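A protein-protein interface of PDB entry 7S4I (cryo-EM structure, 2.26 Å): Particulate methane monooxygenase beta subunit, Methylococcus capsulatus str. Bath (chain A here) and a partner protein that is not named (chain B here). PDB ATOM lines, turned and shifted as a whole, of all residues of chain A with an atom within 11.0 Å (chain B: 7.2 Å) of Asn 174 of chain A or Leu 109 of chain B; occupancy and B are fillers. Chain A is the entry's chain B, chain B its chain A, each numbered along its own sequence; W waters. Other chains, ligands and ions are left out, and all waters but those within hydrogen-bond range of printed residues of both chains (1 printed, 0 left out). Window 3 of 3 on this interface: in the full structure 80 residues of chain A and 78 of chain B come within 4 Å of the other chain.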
ATOM      1  N   PRO A 170       1.626  36.820  16.857  1.00  0.00           N
ATOM      2  CA  PRO A 170       0.951  35.568  17.217  1.00  0.00           C
ATOM      3  C   PRO A 170       0.671  35.492  18.708  1.00  0.00           C
ATOM      4  O   PRO A 170       1.458  35.961  19.534  1.00  0.00           O
ATOM      5  CB  PRO A 170       1.948  34.490  16.781  1.00  0.00           C
ATOM      6  CG  PRO A 170       3.268  35.169  16.832  1.00  0.00           C
ATOM      7  CD  PRO A 170       3.019  36.596  16.439  1.00  0.00           C
ATOM      8  N   VAL A 171      -0.468  34.893  19.045  1.00  0.00           N
ATOM      9  CA  VAL A 171      -0.885  34.712  20.429  1.00  0.00           C
ATOM     10  C   VAL A 171      -1.367  33.280  20.608  1.00  0.00           C
ATOM     11  O   VAL A 171      -2.085  32.743  19.758  1.00  0.00           O
ATOM     12  CB  VAL A 171      -1.993  35.705  20.834  1.00  0.00           C
ATOM     13  CG1 VAL A 171      -2.444  35.439  22.258  1.00  0.00           C
ATOM     14  CG2 VAL A 171      -1.514  37.139  20.685  1.00  0.00           C
ATOM     15  N   GLU A 172      -0.966  32.663  21.715  1.00  0.00           N
ATOM     16  CA  GLU A 172      -1.447  31.337  22.090  1.00  0.00           C
ATOM     17  C   GLU A 172      -2.729  31.531  22.891  1.00  0.00           C
ATOM     18  O   GLU A 172      -2.690  31.848  24.081  1.00  0.00           O
ATOM     19  CB  GLU A 172      -0.384  30.600  22.896  1.00  0.00           C
ATOM     20  CG  GLU A 172      -0.468  29.093  22.832  1.00  0.00           C
ATOM     21  CD  GLU A 172      -1.763  28.557  23.376  1.00  0.00           C
ATOM     22  OE1 GLU A 172      -2.050  28.770  24.574  1.00  0.00           O
ATOM     23  OE2 GLU A 172      -2.503  27.932  22.594  1.00  0.00           O
ATOM     24  N   TYR A 173      -3.875  31.346  22.242  1.00  0.00           N
ATOM     25  CA  TYR A 173      -5.173  31.682  22.826  1.00  0.00           C
ATOM     26  C   TYR A 173      -5.970  30.403  23.063  1.00  0.00           C
ATOM     27  O   TYR A 173      -6.561  29.852  22.130  1.00  0.00           O
ATOM     28  CB  TYR A 173      -5.936  32.647  21.924  1.00  0.00           C
ATOM     29  CG  TYR A 173      -7.105  33.329  22.598  1.00  0.00           C
ATOM     30  CD1 TYR A 173      -6.911  34.430  23.422  1.00  0.00           C
ATOM     31  CD2 TYR A 173      -8.402  32.874  22.408  1.00  0.00           C
ATOM     32  CE1 TYR A 173      -7.976  35.056  24.037  1.00  0.00           C
ATOM     33  CE2 TYR A 173      -9.473  33.495  23.020  1.00  0.00           C
ATOM     34  CZ  TYR A 173      -9.253  34.585  23.833  1.00  0.00           C
ATOM     35  OH  TYR A 173     -10.317  35.205  24.445  1.00  0.00           O
ATOM     36  N   ASN A 174      -5.989  29.947  24.318  1.00  0.00           N
ATOM     37  CA  ASN A 174      -6.807  28.809  24.747  1.00  0.00           C
ATOM     38  C   ASN A 174      -6.553  27.569  23.893  1.00  0.00           C
ATOM     39  O   ASN A 174      -7.481  26.881  23.464  1.00  0.00           O
ATOM     40  CB  ASN A 174      -8.293  29.176  24.745  1.00  0.00           C
ATOM     41  CG  ASN A 174      -8.630  30.242  25.768  1.00  0.00           C
ATOM     42  OD1 ASN A 174      -9.002  31.360  25.416  1.00  0.00           O
ATOM     43  ND2 ASN A 174      -8.505  29.897  27.043  1.00  0.00           N
ATOM     44  N   GLY A 175      -5.278  27.279  23.643  1.00  0.00           N
ATOM     45  CA  GLY A 175      -4.891  26.091  22.915  1.00  0.00           C
ATOM     46  C   GLY A 175      -4.777  26.256  21.416  1.00  0.00           C
ATOM     47  O   GLY A 175      -4.255  25.353  20.749  1.00  0.00           O
ATOM     48  N   MET A 176      -5.237  27.372  20.861  1.00  0.00           N
ATOM     49  CA  MET A 176      -5.215  27.605  19.426  1.00  0.00           C
ATOM     50  C   MET A 176      -4.365  28.829  19.111  1.00  0.00           C
ATOM     51  O   MET A 176      -4.333  29.789  19.887  1.00  0.00           O
ATOM     52  CB  MET A 176      -6.633  27.795  18.881  1.00  0.00           C
ATOM     53  CG  MET A 176      -7.386  26.491  18.660  1.00  0.00           C
ATOM     54  SD  MET A 176      -8.762  26.640  17.505  1.00  0.00           S
ATOM     55  CE  MET A 176      -7.890  26.935  15.971  1.00  0.00           C
ATOM     56  N   LEU A 177      -3.672  28.787  17.977  1.00  0.00           N
ATOM     57  CA  LEU A 177      -2.879  29.926  17.536  1.00  0.00           C
ATOM     58  C   LEU A 177      -3.797  30.959  16.897  1.00  0.00           C
ATOM     59  O   LEU A 177      -4.591  30.629  16.011  1.00  0.00           O
ATOM     60  CB  LEU A 177      -1.796  29.493  16.553  1.00  0.00           C
ATOM     61  CG  LEU A 177      -0.956  30.659  16.020  1.00  0.00           C
ATOM     62  CD1 LEU A 177      -0.047  31.196  17.106  1.00  0.00           C
ATOM     63  CD2 LEU A 177      -0.149  30.261  14.800  1.00  0.00           C
ATOM     64  N   MET A 178      -3.688  32.205  17.347  1.00  0.00           N
ATOM     65  CA  MET A 178      -4.501  33.289  16.822  1.00  0.00           C
ATOM     66  C   MET A 178      -3.671  34.561  16.782  1.00  0.00           C
ATOM     67  O   MET A 178      -2.844  34.809  17.662  1.00  0.00           O
ATOM     68  CB  MET A 178      -5.760  33.514  17.671  1.00  0.00           C
ATOM     69  CG  MET A 178      -6.867  32.501  17.435  1.00  0.00           C
ATOM     70  SD  MET A 178      -8.207  32.649  18.631  1.00  0.00           S
ATOM     71  CE  MET A 178      -9.230  33.889  17.843  1.00  0.00           C
ATOM     72  N   SER A 179      -3.892  35.360  15.745  1.00  0.00           N
ATOM     73  CA  SER A 179      -3.319  36.694  15.713  1.00  0.00           C
ATOM     74  C   SER A 179      -4.136  37.627  16.603  1.00  0.00           C
ATOM     75  O   SER A 179      -5.243  37.302  17.040  1.00  0.00           O
ATOM     76  CB  SER A 179      -3.263  37.219  14.280  1.00  0.00           C
ATOM     77  OG  SER A 179      -4.563  37.469  13.781  1.00  0.00           O
ATOM     78  N   ASP A 182      -7.315  38.386  15.027  1.00  0.00           N
ATOM     79  CA  ASP A 182      -8.218  37.254  15.199  1.00  0.00           C
ATOM     80  C   ASP A 182      -8.887  37.292  16.565  1.00  0.00           C
ATOM     81  O   ASP A 182     -10.096  37.063  16.681  1.00  0.00           O
ATOM     82  CB  ASP A 182      -7.458  35.940  15.018  1.00  0.00           C
ATOM     83  CG  ASP A 182      -7.140  35.642  13.568  1.00  0.00           C
ATOM     84  OD1 ASP A 182      -8.069  35.657  12.736  1.00  0.00           O
ATOM     85  OD2 ASP A 182      -5.955  35.394  13.261  1.00  0.00           O
ATOM     86  N   ILE A 183      -8.114  37.586  17.613  1.00  0.00           N
ATOM     87  CA  ILE A 183      -8.679  37.659  18.956  1.00  0.00           C
ATOM     88  C   ILE A 183      -9.643  38.832  19.070  1.00  0.00           C
ATOM     89  O   ILE A 183     -10.656  38.747  19.769  1.00  0.00           O
ATOM     90  CB  ILE A 183      -7.556  37.740  20.004  1.00  0.00           C
ATOM     91  CG1 ILE A 183      -6.727  36.463  19.978  1.00  0.00           C
ATOM     92  CG2 ILE A 183      -8.128  37.940  21.397  1.00  0.00           C
ATOM     93  CD1 ILE A 183      -5.432  36.588  20.703  1.00  0.00           C
ATOM     94  N   TYR A 186     -12.801  37.688  17.526  1.00  0.00           N
ATOM     95  CA  TYR A 186     -13.429  36.693  18.388  1.00  0.00           C
ATOM     96  C   TYR A 186     -14.103  37.336  19.593  1.00  0.00           C
ATOM     97  O   TYR A 186     -15.261  37.031  19.902  1.00  0.00           O
ATOM     98  CB  TYR A 186     -12.379  35.679  18.837  1.00  0.00           C
ATOM     99  CG  TYR A 186     -12.932  34.490  19.580  1.00  0.00           C
ATOM    100  CD1 TYR A 186     -13.982  33.749  19.062  1.00  0.00           C
ATOM    101  CD2 TYR A 186     -12.392  34.103  20.797  1.00  0.00           C
ATOM    102  CE1 TYR A 186     -14.484  32.659  19.741  1.00  0.00           C
ATOM    103  CE2 TYR A 186     -12.885  33.015  21.480  1.00  0.00           C
ATOM    104  CZ  TYR A 186     -13.930  32.297  20.948  1.00  0.00           C
ATOM    105  OH  TYR A 186     -14.419  31.211  21.631  1.00  0.00           O
ATOM    106  N   ASN A 187     -13.396  38.227  20.285  1.00  0.00           N
ATOM    107  CA  ASN A 187     -13.869  38.824  21.526  1.00  0.00           C
ATOM    108  C   ASN A 187     -15.010  39.799  21.282  1.00  0.00           C
ATOM    109  O   ASN A 187     -16.073  39.685  21.897  1.00  0.00           O
ATOM    110  CB  ASN A 187     -12.723  39.544  22.240  1.00  0.00           C
ATOM    111  CG  ASN A 187     -11.728  38.588  22.862  1.00  0.00           C
ATOM    112  OD1 ASN A 187     -10.672  39.001  23.336  1.00  0.00           O
ATOM    113  ND2 ASN A 187     -12.058  37.304  22.863  1.00  0.00           N
ATOM    114  N   GLU A 195     -18.243  34.465  11.708  1.00  0.00           N
ATOM    115  CA  GLU A 195     -16.870  34.305  11.240  1.00  0.00           C
ATOM    116  C   GLU A 195     -16.812  33.800   9.802  1.00  0.00           C
ATOM    117  O   GLU A 195     -15.909  34.187   9.052  1.00  0.00           O
ATOM    118  CB  GLU A 195     -16.111  33.373  12.195  1.00  0.00           C
ATOM    119  CG  GLU A 195     -14.613  33.167  11.923  1.00  0.00           C
ATOM    120  CD  GLU A 195     -14.311  32.283  10.725  1.00  0.00           C
ATOM    121  OE1 GLU A 195     -15.163  31.440  10.372  1.00  0.00           O
ATOM    122  OE2 GLU A 195     -13.220  32.429  10.138  1.00  0.00           O
ATOM    123  N   LYS B 101     -15.010  35.558  25.598  1.00  0.00           N
ATOM    124  CA  LYS B 101     -13.704  35.060  26.010  1.00  0.00           C
ATOM    125  C   LYS B 101     -13.433  33.687  25.410  1.00  0.00           C
ATOM    126  O   LYS B 101     -12.359  33.434  24.856  1.00  0.00           O
ATOM    127  CB  LYS B 101     -13.619  35.014  27.537  1.00  0.00           C
ATOM    128  CG  LYS B 101     -13.138  36.306  28.172  1.00  0.00           C
ATOM    129  CD  LYS B 101     -11.881  36.830  27.497  1.00  0.00           C
ATOM    130  CE  LYS B 101     -10.685  35.935  27.779  1.00  0.00           C
ATOM    131  NZ  LYS B 101      -9.401  36.575  27.383  1.00  0.00           N
ATOM    132  N   GLU B 102     -14.410  32.787  25.502  1.00  0.00           N
ATOM    133  CA  GLU B 102     -14.262  31.435  24.987  1.00  0.00           C
ATOM    134  C   GLU B 102     -15.610  30.939  24.487  1.00  0.00           C
ATOM    135  O   GLU B 102     -16.668  31.403  24.922  1.00  0.00           O
ATOM    136  CB  GLU B 102     -13.720  30.474  26.051  1.00  0.00           C
ATOM    137  CG  GLU B 102     -12.272  30.699  26.444  1.00  0.00           C
ATOM    138  CD  GLU B 102     -12.078  30.730  27.945  1.00  0.00           C
ATOM    139  OE1 GLU B 102     -12.603  29.827  28.631  1.00  0.00           O
ATOM    140  OE2 GLU B 102     -11.401  31.654  28.441  1.00  0.00           O
ATOM    141  N   SER B 103     -15.557  29.984  23.565  1.00  0.00           N
ATOM    142  CA  SER B 103     -16.748  29.295  23.085  1.00  0.00           C
ATOM    143  C   SER B 103     -16.348  27.874  22.725  1.00  0.00           C
ATOM    144  O   SER B 103     -15.298  27.664  22.113  1.00  0.00           O
ATOM    145  CB  SER B 103     -17.366  30.005  21.877  1.00  0.00           C
ATOM    146  OG  SER B 103     -16.394  30.255  20.878  1.00  0.00           O
ATOM    147  N   TYR B 104     -17.176  26.908  23.109  1.00  0.00           N
ATOM    148  CA  TYR B 104     -16.869  25.502  22.905  1.00  0.00           C
ATOM    149  C   TYR B 104     -18.057  24.788  22.282  1.00  0.00           C
ATOM    150  O   TYR B 104     -19.209  25.066  22.622  1.00  0.00           O
ATOM    151  CB  TYR B 104     -16.497  24.808  24.224  1.00  0.00           C
ATOM    152  CG  TYR B 104     -15.335  25.436  24.952  1.00  0.00           C
ATOM    153  CD1 TYR B 104     -15.526  26.510  25.808  1.00  0.00           C
ATOM    154  CD2 TYR B 104     -14.044  24.957  24.782  1.00  0.00           C
ATOM    155  CE1 TYR B 104     -14.469  27.085  26.475  1.00  0.00           C
ATOM    156  CE2 TYR B 104     -12.978  25.528  25.445  1.00  0.00           C
ATOM    157  CZ  TYR B 104     -13.196  26.593  26.289  1.00  0.00           C
ATOM    158  OH  TYR B 104     -12.140  27.167  26.953  1.00  0.00           O
ATOM    159  N   ILE B 105     -17.768  23.876  21.361  1.00  0.00           N
ATOM    160  CA  ILE B 105     -18.732  22.899  20.875  1.00  0.00           C
ATOM    161  C   ILE B 105     -18.153  21.527  21.179  1.00  0.00           C
ATOM    162  O   ILE B 105     -17.063  21.187  20.703  1.00  0.00           O
ATOM    163  CB  ILE B 105     -19.022  23.067  19.377  1.00  0.00           C
ATOM    164  CG1 ILE B 105     -19.673  24.427  19.111  1.00  0.00           C
ATOM    165  CG2 ILE B 105     -19.901  21.928  18.877  1.00  0.00           C
ATOM    166  CD1 ILE B 105     -20.396  24.517  17.786  1.00  0.00           C
ATOM    167  N   GLY B 106     -18.871  20.743  21.972  1.00  0.00           N
ATOM    168  CA  GLY B 106     -18.302  19.518  22.491  1.00  0.00           C
ATOM    169  C   GLY B 106     -17.507  19.812  23.745  1.00  0.00           C
ATOM    170  O   GLY B 106     -18.078  19.988  24.825  1.00  0.00           O
ATOM    171  N   GLY B 107     -16.186  19.865  23.613  1.00  0.00           N
ATOM    172  CA  GLY B 107     -15.333  20.281  24.707  1.00  0.00           C
ATOM    173  C   GLY B 107     -14.148  21.093  24.228  1.00  0.00           C
ATOM    174  O   GLY B 107     -13.233  21.391  25.001  1.00  0.00           O
ATOM    175  N   GLN B 108     -14.157  21.459  22.950  1.00  0.00           N
ATOM    176  CA  GLN B 108     -13.025  22.098  22.300  1.00  0.00           C
ATOM    177  C   GLN B 108     -13.390  23.498  21.822  1.00  0.00           C
ATOM    178  O   GLN B 108     -14.526  23.752  21.413  1.00  0.00           O
ATOM    179  CB  GLN B 108     -12.532  21.240  21.134  1.00  0.00           C
ATOM    180  CG  GLN B 108     -13.546  21.056  20.030  1.00  0.00           C
ATOM    181  CD  GLN B 108     -12.918  21.101  18.660  1.00  0.00           C
ATOM    182  OE1 GLN B 108     -12.610  22.173  18.145  1.00  0.00           O
ATOM    183  NE2 GLN B 108     -12.720  19.933  18.059  1.00  0.00           N
ATOM    184  N   LEU B 109     -12.414  24.403  21.885  1.00  0.00           N
ATOM    185  CA  LEU B 109     -12.647  25.800  21.548  1.00  0.00           C
ATOM    186  C   LEU B 109     -12.948  25.960  20.064  1.00  0.00           C
ATOM    187  O   LEU B 109     -12.342  25.303  19.214  1.00  0.00           O
ATOM    188  CB  LEU B 109     -11.430  26.638  21.939  1.00  0.00           C
ATOM    189  CG  LEU B 109     -11.587  28.157  21.894  1.00  0.00           C
ATOM    190  CD1 LEU B 109     -11.920  28.695  23.275  1.00  0.00           C
ATOM    191  CD2 LEU B 109     -10.324  28.805  21.355  1.00  0.00           C
ATOM    192  N   VAL B 110     -13.886  26.849  19.751  1.00  0.00           N
ATOM    193  CA  VAL B 110     -14.336  27.031  18.373  1.00  0.00           C
ATOM    194  C   VAL B 110     -14.295  28.508  17.992  1.00  0.00           C
ATOM    195  O   VAL B 110     -15.348  29.131  17.801  1.00  0.00           O
ATOM    196  CB  VAL B 110     -15.740  26.436  18.174  1.00  0.00           C
ATOM    197  CG1 VAL B 110     -15.657  24.925  18.113  1.00  0.00           C
ATOM    198  CG2 VAL B 110     -16.669  26.851  19.307  1.00  0.00           C
ATOM    199  N   PRO B 111     -13.110  29.110  17.850  1.00  0.00           N
ATOM    200  CA  PRO B 111     -13.053  30.513  17.419  1.00  0.00           C
ATOM    201  C   PRO B 111     -13.366  30.710  15.949  1.00  0.00           C
ATOM    202  O   PRO B 111     -13.534  31.859  15.520  1.00  0.00           O
ATOM    203  CB  PRO B 111     -11.608  30.916  17.733  1.00  0.00           C
ATOM    204  CG  PRO B 111     -10.847  29.650  17.578  1.00  0.00           C
ATOM    205  CD  PRO B 111     -11.764  28.533  18.015  1.00  0.00           C
ATOM    206  N   ARG B 112     -13.445  29.640  15.169  1.00  0.00           N
ATOM    207  CA  ARG B 112     -13.735  29.700  13.747  1.00  0.00           C
ATOM    208  C   ARG B 112     -15.064  29.005  13.466  1.00  0.00           C
ATOM    209  O   ARG B 112     -15.715  28.465  14.364  1.00  0.00           O
ATOM    210  CB  ARG B 112     -12.600  29.066  12.942  1.00  0.00           C
ATOM    211  CG  ARG B 112     -11.212  29.396  13.462  1.00  0.00           C
ATOM    212  CD  ARG B 112     -10.185  29.334  12.352  1.00  0.00           C
ATOM    213  NE  ARG B 112      -8.906  28.802  12.805  1.00  0.00           N
ATOM    214  CZ  ARG B 112      -8.320  27.729  12.293  1.00  0.00           C
ATOM    215  NH1 ARG B 112      -8.882  27.032  11.321  1.00  0.00           N
ATOM    216  NH2 ARG B 112      -7.136  27.350  12.766  1.00  0.00           N
ATOM    217  N   VAL B 114     -17.547  26.090  12.144  1.00  0.00           N
ATOM    218  CA  VAL B 114     -17.486  24.656  12.379  1.00  0.00           C
ATOM    219  C   VAL B 114     -18.501  23.958  11.486  1.00  0.00           C
ATOM    220  O   VAL B 114     -19.431  24.569  10.955  1.00  0.00           O
ATOM    221  CB  VAL B 114     -17.733  24.293  13.856  1.00  0.00           C
ATOM    222  CG1 VAL B 114     -16.753  25.024  14.747  1.00  0.00           C
ATOM    223  CG2 VAL B 114     -19.164  24.611  14.250  1.00  0.00           C
ATOM    224  N   ARG B 125     -20.696  25.666  25.223  1.00  0.00           N
ATOM    225  CA  ARG B 125     -20.369  26.480  26.387  1.00  0.00           C
ATOM    226  C   ARG B 125     -19.734  27.770  25.896  1.00  0.00           C
ATOM    227  O   ARG B 125     -18.708  27.733  25.211  1.00  0.00           O
ATOM    228  CB  ARG B 125     -19.427  25.733  27.330  1.00  0.00           C
ATOM    229  CG  ARG B 125     -18.919  26.562  28.492  1.00  0.00           C
ATOM    230  CD  ARG B 125     -18.327  25.669  29.566  1.00  0.00           C
ATOM    231  NE  ARG B 125     -16.954  25.288  29.258  1.00  0.00           N
ATOM    232  CZ  ARG B 125     -15.884  25.971  29.637  1.00  0.00           C
ATOM    233  NH1 ARG B 125     -15.986  27.075  30.358  1.00  0.00           N
ATOM    234  NH2 ARG B 125     -14.678  25.532  29.288  1.00  0.00           N
ATOM    235  N   MET B 269     -13.672  24.434  10.859  1.00  0.00           N
ATOM    236  CA  MET B 269     -13.098  23.361  11.656  1.00  0.00           C
ATOM    237  C   MET B 269     -14.033  22.159  11.620  1.00  0.00           C
ATOM    238  O   MET B 269     -15.205  22.265  11.994  1.00  0.00           O
ATOM    239  CB  MET B 269     -12.866  23.828  13.091  1.00  0.00           C
ATOM    240  CG  MET B 269     -11.677  24.762  13.236  1.00  0.00           C
ATOM    241  SD  MET B 269     -11.599  25.553  14.851  1.00  0.00           S
ATOM    242  CE  MET B 269     -11.678  24.125  15.917  1.00  0.00           C
ATOM    243  N   MET B 272     -16.316  18.103  14.800  1.00  0.00           N
ATOM    244  CA  MET B 272     -17.001  18.461  16.037  1.00  0.00           C
ATOM    245  C   MET B 272     -17.549  17.184  16.660  1.00  0.00           C
ATOM    246  O   MET B 272     -18.191  16.382  15.978  1.00  0.00           O
ATOM    247  CB  MET B 272     -18.116  19.469  15.774  1.00  0.00           C
ATOM    248  CG  MET B 272     -17.661  20.794  15.177  1.00  0.00           C
ATOM    249  SD  MET B 272     -16.620  21.774  16.281  1.00  0.00           S
ATOM    250  CE  MET B 272     -14.976  21.320  15.731  1.00  0.00           C
HETATM  251  O   HOH W   1      -4.919  28.610  14.054  1.00  0.00           O
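O of Lys 101 of chain B touches OD1 of Asn 174 of chain A, at 3.99 Å.
Asn 174 of chain A touches Glu 102 of chain B (OD1 to CG, 3.5 Å).
CB of Asn 174 of chain A touches CD1 of Leu 109 of chain B, 3.9 Å away.
Met 176 of chain A touches Pro 111 of chain B.
Tyr 186 of chain A touches Lys 101 of chain B (CE2 to O, 3.4 Å).
Glu 102 of chain B touches Tyr 186 of chain A (C to OH, 3.1 Å).
Leu 109 of chain B touches Tyr 186 of chain A (CD1 to OH, 3.9 Å).
CA of Pro 111 of chain B touches CE1 of Tyr 186 of chain A, at 3.5 Å.
Glu 195 of chain A touches Pro 111 of chain B.
OE1 of Glu 195 of chain A touches C of Arg 112 of chain B (3.9 Å).
OE1 of Glu 102 of chain B is in hydrogen-bond range of OH of Tyr 104 of chain B (3.2 Å).
O of Ser 103 of chain B is in hydrogen-bond range of N of Val 110 of chain B, at 2.9 Å.
N of Val 171 of chain A lies within hydrogen-bond range of O of Met 178 of chain A (2.8 Å).
The backbone NH (N) of Met 176 of chain A is in hydrogen-bond range of the side-chain carboxylate (OE2) of Glu 172 of chain A.
OH of Tyr 173 of chain A is in hydrogen-bond range of ND2 of Asn 187 of chain A, 3.2 Å away.
OH of Tyr 173 of chain A lies within hydrogen-bond range of O of Lys 101 of chain B (2.7 Å).
OH of Tyr 186 of chain A lies within hydrogen-bond range of N of Ser 103 of chain B (2.6 Å).
Of the printed residues of chain B, Tyr 173 of chain A touches Lys 101 (2.7 Å) and Leu 109 (3.98 Å).
Of the printed residues of chain B, Asn 174 of chain A touches Lys 101 (3.99 Å), Glu 102 (3.5 Å) and Leu 109 (3.9 Å).
Of the printed residues of chain B, Met 176 of chain A touches Pro 111 and Arg 112.
Printed residues of chain B within 4 Å of Met 178 of chain A: Pro 111 (3.8 Å).
Of the printed residues of chain B, Glu 195 of chain A touches Pro 111 and Arg 112.
Glu 102 of chain B touches just these residues of chain A: Asn 174 (3.5 Å) and Tyr 186 (3.1 Å).
Ser 103 of chain B touches just one residue of chain A: Tyr 186.
No residue of chain A comes within 4 Å of Tyr 104 of chain B.
No residue of chain A comes within 4 Å of Gln 108 of chain B.
Of the printed residues of chain A, Leu 109 of chain B touches Tyr 173 (3.98 Å), Asn 174 (3.9 Å) and Tyr 186 (3.9 Å).
No residue of chain A comes within 4 Å of Val 110 of chain B.
Of the printed residues of chain A, Arg 112 of chain B touches Met 176 (3.3 Å) and Glu 195 (3.9 Å).
The nearest printed residue of chain B that does not touch Asn 174 of chain A is Tyr 104 of chain B (4.5 Å).
The nearest printed residue of chain A that does not touch Leu 109 of chain B is Met 176 of chain A (4.2 Å).
Water W1 bridges O of Leu 177 of chain A (2.8 Å) and NH2 of Arg 112 of chain B (2.9 Å).
Hydrophobic or aromatic side chains of chain B within 4 Å of the printed part of chain A: Leu 109 and Pro 111.
Hydrophobic or aromatic side chains of chain A within 4 Å of the printed part of chain B: Tyr 173, Met 176, Met 178 and Tyr 186.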
